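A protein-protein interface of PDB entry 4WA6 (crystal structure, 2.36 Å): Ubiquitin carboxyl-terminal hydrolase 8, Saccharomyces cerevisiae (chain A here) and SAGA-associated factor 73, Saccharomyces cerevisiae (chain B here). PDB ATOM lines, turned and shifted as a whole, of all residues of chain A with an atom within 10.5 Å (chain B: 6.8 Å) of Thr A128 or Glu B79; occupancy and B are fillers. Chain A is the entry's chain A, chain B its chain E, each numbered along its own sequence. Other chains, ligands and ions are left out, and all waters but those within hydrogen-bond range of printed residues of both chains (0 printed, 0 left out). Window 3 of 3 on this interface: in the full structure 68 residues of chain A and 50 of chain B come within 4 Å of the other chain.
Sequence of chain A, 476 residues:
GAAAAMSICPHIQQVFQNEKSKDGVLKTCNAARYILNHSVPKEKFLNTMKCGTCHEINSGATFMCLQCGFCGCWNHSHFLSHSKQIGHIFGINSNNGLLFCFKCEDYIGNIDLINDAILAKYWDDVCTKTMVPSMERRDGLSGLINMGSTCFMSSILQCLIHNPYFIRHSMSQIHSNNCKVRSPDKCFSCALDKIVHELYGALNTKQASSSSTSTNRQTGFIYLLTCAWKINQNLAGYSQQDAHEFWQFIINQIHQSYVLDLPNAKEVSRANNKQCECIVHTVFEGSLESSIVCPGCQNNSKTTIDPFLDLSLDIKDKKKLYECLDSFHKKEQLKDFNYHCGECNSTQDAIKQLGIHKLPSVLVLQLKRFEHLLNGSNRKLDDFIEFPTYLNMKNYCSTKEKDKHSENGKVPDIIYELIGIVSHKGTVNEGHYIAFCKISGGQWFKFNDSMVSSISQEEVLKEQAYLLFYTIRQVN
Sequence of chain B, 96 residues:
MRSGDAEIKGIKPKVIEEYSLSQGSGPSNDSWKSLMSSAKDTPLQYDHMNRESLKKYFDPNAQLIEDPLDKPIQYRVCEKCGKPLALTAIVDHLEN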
ATOM      1  N   TYR A 122       4.413   4.457  -4.131  1.00  0.00           N
ATOM      2  CA  TYR A 122       4.571   5.474  -3.095  1.00  0.00           C
ATOM      3  C   TYR A 122       4.500   6.867  -3.682  1.00  0.00           C
ATOM      4  O   TYR A 122       4.921   7.867  -3.072  1.00  0.00           O
ATOM      5  CB  TYR A 122       5.940   5.288  -2.454  1.00  0.00           C
ATOM      6  CG  TYR A 122       6.151   3.939  -1.824  1.00  0.00           C
ATOM      7  CD1 TYR A 122       5.631   3.666  -0.574  1.00  0.00           C
ATOM      8  CD2 TYR A 122       6.865   2.930  -2.482  1.00  0.00           C
ATOM      9  CE1 TYR A 122       5.815   2.441   0.024  1.00  0.00           C
ATOM     10  CE2 TYR A 122       7.066   1.693  -1.888  1.00  0.00           C
ATOM     11  CZ  TYR A 122       6.543   1.467  -0.627  1.00  0.00           C
ATOM     12  OH  TYR A 122       6.715   0.264   0.011  1.00  0.00           O
ATOM     13  N   TRP A 123       3.947   6.942  -4.867  1.00  0.00           N
ATOM     14  CA  TRP A 123       4.202   8.084  -5.697  1.00  0.00           C
ATOM     15  C   TRP A 123       3.633   9.412  -5.136  1.00  0.00           C
ATOM     16  O   TRP A 123       4.294  10.441  -5.210  1.00  0.00           O
ATOM     17  CB  TRP A 123       3.776   7.813  -7.158  1.00  0.00           C
ATOM     18  CG  TRP A 123       4.358   8.861  -8.084  1.00  0.00           C
ATOM     19  CD1 TRP A 123       3.675   9.819  -8.769  1.00  0.00           C
ATOM     20  CD2 TRP A 123       5.749   9.113  -8.328  1.00  0.00           C
ATOM     21  NE1 TRP A 123       4.550  10.629  -9.436  1.00  0.00           N
ATOM     22  CE2 TRP A 123       5.825  10.220  -9.186  1.00  0.00           C
ATOM     23  CE3 TRP A 123       6.931   8.497  -7.914  1.00  0.00           C
ATOM     24  CZ2 TRP A 123       7.035  10.720  -9.662  1.00  0.00           C
ATOM     25  CZ3 TRP A 123       8.122   8.991  -8.375  1.00  0.00           C
ATOM     26  CH2 TRP A 123       8.163  10.108  -9.242  1.00  0.00           C
ATOM     27  N   ASP A 124       2.445   9.407  -4.554  1.00  0.00           N
ATOM     28  CA  ASP A 124       1.885  10.659  -4.039  1.00  0.00           C
ATOM     29  C   ASP A 124       2.747  11.294  -2.933  1.00  0.00           C
ATOM     30  O   ASP A 124       2.849  12.509  -2.815  1.00  0.00           O
ATOM     31  CB  ASP A 124       0.468  10.430  -3.499  1.00  0.00           C
ATOM     32  CG  ASP A 124      -0.526  10.055  -4.590  1.00  0.00           C
ATOM     33  OD1 ASP A 124      -0.370  10.526  -5.736  1.00  0.00           O
ATOM     34  OD2 ASP A 124      -1.486   9.307  -4.289  1.00  0.00           O
ATOM     35  N   ASP A 125       3.348  10.447  -2.121  1.00  0.00           N
ATOM     36  CA  ASP A 125       4.230  10.896  -1.071  1.00  0.00           C
ATOM     37  C   ASP A 125       5.515  11.441  -1.614  1.00  0.00           C
ATOM     38  O   ASP A 125       5.952  12.522  -1.177  1.00  0.00           O
ATOM     39  CB  ASP A 125       4.490   9.762  -0.106  1.00  0.00           C
ATOM     40  CG  ASP A 125       3.321   9.541   0.812  1.00  0.00           C
ATOM     41  OD1 ASP A 125       3.191  10.337   1.754  1.00  0.00           O
ATOM     42  OD2 ASP A 125       2.513   8.613   0.582  1.00  0.00           O
ATOM     43  N   VAL A 126       6.095  10.715  -2.579  1.00  0.00           N
ATOM     44  CA  VAL A 126       7.369  11.100  -3.204  1.00  0.00           C
ATOM     45  C   VAL A 126       7.203  12.420  -3.942  1.00  0.00           C
ATOM     46  O   VAL A 126       8.121  13.254  -3.951  1.00  0.00           O
ATOM     47  CB  VAL A 126       7.883  10.026  -4.207  1.00  0.00           C
ATOM     48  CG1 VAL A 126       8.989  10.592  -5.100  1.00  0.00           C
ATOM     49  CG2 VAL A 126       8.357   8.777  -3.474  1.00  0.00           C
ATOM     50  N   CYS A 127       6.039  12.605  -4.560  1.00  0.00           N
ATOM     51  CA  CYS A 127       5.701  13.858  -5.228  1.00  0.00           C
ATOM     52  C   CYS A 127       5.618  15.089  -4.359  1.00  0.00           C
ATOM     53  O   CYS A 127       6.060  16.167  -4.739  1.00  0.00           O
ATOM     54  CB  CYS A 127       4.340  13.719  -5.880  1.00  0.00           C
ATOM     55  SG  CYS A 127       4.670  13.038  -7.472  1.00  0.00           S
ATOM     56  N   THR A 128       4.978  14.930  -3.222  1.00  0.00           N
ATOM     57  CA  THR A 128       4.637  16.054  -2.408  1.00  0.00           C
ATOM     58  C   THR A 128       5.766  16.341  -1.420  1.00  0.00           C
ATOM     59  O   THR A 128       5.907  17.456  -0.975  1.00  0.00           O
ATOM     60  CB  THR A 128       3.294  15.798  -1.696  1.00  0.00           C
ATOM     61  OG1 THR A 128       3.367  14.573  -0.958  1.00  0.00           O
ATOM     62  CG2 THR A 128       2.194  15.672  -2.722  1.00  0.00           C
ATOM     63  N   LYS A 129       6.595  15.355  -1.117  1.00  0.00           N
ATOM     64  CA  LYS A 129       7.639  15.538  -0.117  1.00  0.00           C
ATOM     65  C   LYS A 129       9.060  15.659  -0.649  1.00  0.00           C
ATOM     66  O   LYS A 129       9.955  16.070   0.094  1.00  0.00           O
ATOM     67  CB  LYS A 129       7.591  14.389   0.872  1.00  0.00           C
ATOM     68  CG  LYS A 129       6.238  14.277   1.544  1.00  0.00           C
ATOM     69  CD  LYS A 129       6.309  13.288   2.683  1.00  0.00           C
ATOM     70  CE  LYS A 129       4.971  12.602   2.873  1.00  0.00           C
ATOM     71  NZ  LYS A 129       4.776  12.247   4.304  1.00  0.00           N
ATOM     72  N   THR A 130       9.288  15.291  -1.909  1.00  0.00           N
ATOM     73  CA  THR A 130      10.578  15.517  -2.532  1.00  0.00           C
ATOM     74  C   THR A 130      10.392  16.272  -3.826  1.00  0.00           C
ATOM     75  O   THR A 130       9.343  16.223  -4.425  1.00  0.00           O
ATOM     76  CB  THR A 130      11.336  14.203  -2.820  1.00  0.00           C
ATOM     77  OG1 THR A 130      10.597  13.403  -3.731  1.00  0.00           O
ATOM     78  CG2 THR A 130      11.523  13.414  -1.590  1.00  0.00           C
ATOM     79  N   MET A 131      11.445  16.945  -4.253  1.00  0.00           N
ATOM     80  CA  MET A 131      11.458  17.711  -5.467  1.00  0.00           C
ATOM     81  C   MET A 131      12.650  17.294  -6.364  1.00  0.00           C
ATOM     82  O   MET A 131      13.641  16.688  -5.911  1.00  0.00           O
ATOM     83  CB  MET A 131      11.519  19.210  -5.126  1.00  0.00           C
ATOM     84  CG  MET A 131      12.793  19.688  -4.420  1.00  0.00           C
ATOM     85  SD  MET A 131      12.494  21.278  -3.629  1.00  0.00           S
ATOM     86  CE  MET A 131      13.748  21.340  -2.363  1.00  0.00           C
ATOM     87  N   VAL A 132      12.542  17.622  -7.641  1.00  0.00           N
ATOM     88  CA  VAL A 132      13.623  17.385  -8.561  1.00  0.00           C
ATOM     89  C   VAL A 132      14.784  18.334  -8.255  1.00  0.00           C
ATOM     90  O   VAL A 132      14.621  19.367  -7.650  1.00  0.00           O
ATOM     91  CB  VAL A 132      13.167  17.533 -10.025  1.00  0.00           C
ATOM     92  CG1 VAL A 132      12.011  16.557 -10.313  1.00  0.00           C
ATOM     93  CG2 VAL A 132      12.789  18.986 -10.356  1.00  0.00           C
ATOM     94  N   PRO A 133      15.974  17.973  -8.667  1.00  0.00           N
ATOM     95  CA  PRO A 133      17.067  18.881  -8.382  1.00  0.00           C
ATOM     96  C   PRO A 133      16.830  20.281  -8.939  1.00  0.00           C
ATOM     97  O   PRO A 133      16.143  20.469  -9.926  1.00  0.00           O
ATOM     98  CB  PRO A 133      18.256  18.223  -9.108  1.00  0.00           C
ATOM     99  CG  PRO A 133      17.863  16.807  -9.371  1.00  0.00           C
ATOM    100  CD  PRO A 133      16.399  16.650  -9.139  1.00  0.00           C
ATOM    101  N   SER A 134      17.411  21.272  -8.326  1.00  0.00           N
ATOM    102  CA  SER A 134      17.358  22.573  -8.890  1.00  0.00           C
ATOM    103  C   SER A 134      18.394  22.593 -10.031  1.00  0.00           C
ATOM    104  O   SER A 134      19.446  21.911  -9.978  1.00  0.00           O
ATOM    105  CB  SER A 134      17.664  23.624  -7.840  1.00  0.00           C
ATOM    106  OG  SER A 134      19.039  23.578  -7.524  1.00  0.00           O
ATOM    107  N   HIS A 197      25.390  16.978   0.286  1.00  0.00           N
ATOM    108  CA  HIS A 197      24.143  17.710   0.628  1.00  0.00           C
ATOM    109  C   HIS A 197      24.153  19.158   0.098  1.00  0.00           C
ATOM    110  O   HIS A 197      23.254  19.555  -0.639  1.00  0.00           O
ATOM    111  CB  HIS A 197      23.967  17.691   2.133  1.00  0.00           C
ATOM    112  CG  HIS A 197      22.620  18.135   2.619  1.00  0.00           C
ATOM    113  ND1 HIS A 197      22.202  17.912   3.921  1.00  0.00           N
ATOM    114  CD2 HIS A 197      21.610  18.804   2.013  1.00  0.00           C
ATOM    115  CE1 HIS A 197      20.991  18.410   4.088  1.00  0.00           C
ATOM    116  NE2 HIS A 197      20.615  18.974   2.955  1.00  0.00           N
ATOM    117  N   GLY A 201      21.879  19.106  -3.093  1.00  0.00           N
ATOM    118  CA  GLY A 201      20.537  19.564  -2.626  1.00  0.00           C
ATOM    119  C   GLY A 201      20.604  20.974  -2.052  1.00  0.00           C
ATOM    120  O   GLY A 201      21.201  21.823  -2.673  1.00  0.00           O
ATOM    121  N   ALA A 202      20.051  21.198  -0.850  1.00  0.00           N
ATOM    122  CA  ALA A 202      20.116  22.503  -0.138  1.00  0.00           C
ATOM    123  C   ALA A 202      20.207  22.304   1.384  1.00  0.00           C
ATOM    124  O   ALA A 202      19.397  21.585   1.951  1.00  0.00           O
ATOM    125  CB  ALA A 202      18.903  23.375  -0.467  1.00  0.00           C
ATOM    126  N   LEU A 203      21.160  22.985   2.033  1.00  0.00           N
ATOM    127  CA  LEU A 203      21.574  22.701   3.430  1.00  0.00           C
ATOM    128  C   LEU A 203      21.063  23.704   4.451  1.00  0.00           C
ATOM    129  O   LEU A 203      19.869  23.988   4.516  1.00  0.00           O
ATOM    130  CB  LEU A 203      23.108  22.652   3.497  1.00  0.00           C
ATOM    131  CG  LEU A 203      23.805  22.382   4.842  1.00  0.00           C
ATOM    132  CD1 LEU A 203      23.434  21.008   5.386  1.00  0.00           C
ATOM    133  CD2 LEU A 203      25.326  22.489   4.721  1.00  0.00           C
ATOM    134  N   ARG B  76      16.210  12.850  -5.965  1.00  0.00           N
ATOM    135  CA  ARG B  76      15.324  13.899  -5.621  1.00  0.00           C
ATOM    136  C   ARG B  76      15.707  14.360  -4.265  1.00  0.00           C
ATOM    137  O   ARG B  76      16.335  13.626  -3.505  1.00  0.00           O
ATOM    138  CB  ARG B  76      13.907  13.400  -5.623  1.00  0.00           C
ATOM    139  CG  ARG B  76      13.466  12.922  -6.999  1.00  0.00           C
ATOM    140  CD  ARG B  76      12.108  12.278  -6.865  1.00  0.00           C
ATOM    141  NE  ARG B  76      11.078  13.241  -6.489  1.00  0.00           N
ATOM    142  CZ  ARG B  76      10.415  14.015  -7.349  1.00  0.00           C
ATOM    143  NH1 ARG B  76      10.654  13.974  -8.665  1.00  0.00           N
ATOM    144  NH2 ARG B  76       9.484  14.806  -6.891  1.00  0.00           N
ATOM    145  N   VAL B  77      15.328  15.605  -3.994  1.00  0.00           N
ATOM    146  CA  VAL B  77      15.805  16.374  -2.860  1.00  0.00           C
ATOM    147  C   VAL B  77      14.606  16.469  -1.922  1.00  0.00           C
ATOM    148  O   VAL B  77      13.504  16.849  -2.340  1.00  0.00           O
ATOM    149  CB  VAL B  77      16.191  17.793  -3.319  1.00  0.00           C
ATOM    150  CG1 VAL B  77      16.451  18.709  -2.148  1.00  0.00           C
ATOM    151  CG2 VAL B  77      17.391  17.791  -4.244  1.00  0.00           C
ATOM    152  N   CYS B  78      14.811  16.111  -0.667  1.00  0.00           N
ATOM    153  CA  CYS B  78      13.786  16.259   0.366  1.00  0.00           C
ATOM    154  C   CYS B  78      13.439  17.733   0.645  1.00  0.00           C
ATOM    155  O   CYS B  78      14.305  18.544   0.914  1.00  0.00           O
ATOM    156  CB  CYS B  78      14.235  15.544   1.643  1.00  0.00           C
ATOM    157  SG  CYS B  78      13.135  15.724   3.054  1.00  0.00           S
ATOM    158  N   GLU B  79      12.148  18.064   0.563  1.00  0.00           N
ATOM    159  CA  GLU B  79      11.671  19.427   0.833  1.00  0.00           C
ATOM    160  C   GLU B  79      11.774  19.787   2.291  1.00  0.00           C
ATOM    161  O   GLU B  79      11.861  20.940   2.612  1.00  0.00           O
ATOM    162  CB  GLU B  79      10.219  19.595   0.380  1.00  0.00           C
ATOM    163  CG  GLU B  79      10.051  19.524  -1.127  1.00  0.00           C
ATOM    164  CD  GLU B  79       8.686  19.975  -1.568  1.00  0.00           C
ATOM    165  OE1 GLU B  79       8.290  21.100  -1.199  1.00  0.00           O
ATOM    166  OE2 GLU B  79       8.006  19.209  -2.284  1.00  0.00           O
ATOM    167  N   LYS B  80      11.787  18.804   3.177  1.00  0.00           N
ATOM    168  CA  LYS B  80      11.972  19.088   4.591  1.00  0.00           C
ATOM    169  C   LYS B  80      13.430  19.489   4.925  1.00  0.00           C
ATOM    170  O   LYS B  80      13.662  20.560   5.469  1.00  0.00           O
ATOM    171  CB  LYS B  80      11.546  17.891   5.440  1.00  0.00           C
ATOM    172  CG  LYS B  80      10.586  18.254   6.555  1.00  0.00           C
ATOM    173  CD  LYS B  80       9.138  18.220   6.068  1.00  0.00           C
ATOM    174  CE  LYS B  80       8.216  18.944   7.031  1.00  0.00           C
ATOM    175  NZ  LYS B  80       6.826  19.025   6.502  1.00  0.00           N
ATOM    176  N   CYS B  81      14.416  18.649   4.604  1.00  0.00           N
ATOM    177  CA  CYS B  81      15.812  18.915   5.044  1.00  0.00           C
ATOM    178  C   CYS B  81      16.794  19.233   3.895  1.00  0.00           C
ATOM    179  O   CYS B  81      17.951  19.542   4.120  1.00  0.00           O
ATOM    180  CB  CYS B  81      16.325  17.734   5.838  1.00  0.00           C
ATOM    181  SG  CYS B  81      16.525  16.307   4.777  1.00  0.00           S
ATOM    182  N   GLY B  82      16.323  19.153   2.663  1.00  0.00           N
ATOM    183  CA  GLY B  82      17.147  19.475   1.503  1.00  0.00           C
ATOM    184  C   GLY B  82      18.110  18.394   1.027  1.00  0.00           C
ATOM    185  O   GLY B  82      18.904  18.655   0.117  1.00  0.00           O
ATOM    186  N   LYS B  83      18.080  17.211   1.651  1.00  0.00           N
ATOM    187  CA  LYS B  83      19.063  16.174   1.339  1.00  0.00           C
ATOM    188  C   LYS B  83      18.823  15.588  -0.040  1.00  0.00           C
ATOM    189  O   LYS B  83      17.690  15.211  -0.354  1.00  0.00           O
ATOM    190  CB  LYS B  83      19.008  14.992   2.295  1.00  0.00           C
ATOM    191  CG  LYS B  83      19.962  15.115   3.457  1.00  0.00           C
ATOM    192  CD  LYS B  83      19.606  14.155   4.576  1.00  0.00           C
ATOM    193  CE  LYS B  83      20.493  14.412   5.766  1.00  0.00           C
ATOM    194  NZ  LYS B  83      20.588  13.188   6.609  1.00  0.00           N
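The backbone carbonyl oxygen of Lys A129 is in hydrogen-bond range of the backbone NH of Glu B79, at 3.0 Å.
OG1 of Thr A130 is in hydrogen-bond range of NE of Arg B76 (2.8 Å).
The backbone NH (N) of Val B77 is in hydrogen-bond range of the backbone carbonyl oxygen (O) of Met A131, at 2.8 Å.
A ring nitrogen (NE2) of His A197 is in hydrogen-bond range of the backbone carbonyl oxygen (O) of Cys B81 (3.0 Å).
A ring nitrogen (NE2) of His A197 lies close to the backbone carbonyl oxygen of Gly B82 (3.3 Å).
A ring nitrogen (NE2) of His A197 sits at hydrogen-bond distance from the backbone NH (N) of Lys B83 (3.4 Å).
The backbone carbonyl oxygen (O) of Gly B82 sits at hydrogen-bond distance from the backbone NH (N) of Ala A202.
O of Thr A128 lies close to OE2 of Glu B79 (3.0 Å).
The backbone carbonyl oxygen (O) of Ala A202 sits close to the backbone carbonyl oxygen (O) of Cys B81, 3.3 Å away.
Hydrophobic or aromatic side chains of chain A within 4 Å of the printed part of chain B: Val A126, Met A131, Val A132 and His A197.
Along chain A the printed residues that touch a printed residue of chain B span positions 126 to 202.
The backbone carbonyl oxygen of Asp A124 is in hydrogen-bond range of the side-chain hydroxyl of Thr A128.
NZ of Lys A129 lies within salt-bridge range of OD1 of Asp A125, at 3.6 Å.
OG1 of Thr A130 is in hydrogen-bond range of O of Val A126, at 2.5 Å.
A ring nitrogen (NE2) of His A197 lies within hydrogen-bond range of the backbone carbonyl oxygen of Ala A202.
N of Cys B78 lies within hydrogen-bond range of O of Lys B83, at 3.0 Å.
SG of Cys B81 lies close to N of Lys B83 (3.6 Å).
Thr A128 touches just one residue of chain B: Glu B79 (3.0 Å).
Of the printed residues of chain B, Lys A129 touches Cys B78 and Glu B79.
Printed residues of chain B within 4 Å of Thr A130: Arg B76, Val B77 and Glu B79.
Of the printed residues of chain B, Met A131 touches Arg B76, Val B77 and Glu B79.
Pro A133 touches none of the printed residues of chain B.
Printed residues of chain A within 4 Å of Arg B76: Val A126, Thr A130, Met A131 and Val A132.
Glu B79 touches just these residues of chain A: Thr A128, Lys A129, Thr A130 and Met A131.
Printed residues of chain A within 4 Å of Gly B82: His A197 (3.2 Å), Gly A201 (3.3 Å) and Ala A202 (3.0 Å).
The nearest residue of chain A that does not touch Glu B79 is Cys A127 (4.4 Å).
The nearest printed residue of chain B that does not touch Thr A130 is Cys B78 (4.1 Å).
Among the printed residues, pairs that only touch across the chains: Thr A130 with Val B77 (3.2 Å), Met A131 with Arg B76 (3.3 Å), Gly A201 with Gly B82 (3.3 Å), Val A132 with Arg B76 (3.4 Å), Val A126 with Arg B76 (3.6 Å), Lys A129 with Cys B78 (3.8 Å), Thr A130 with Glu B79 (3.9 Å), Met A131 with Glu B79 (3.9 Å) and Gly A201 with Val B77 (3.96 Å).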
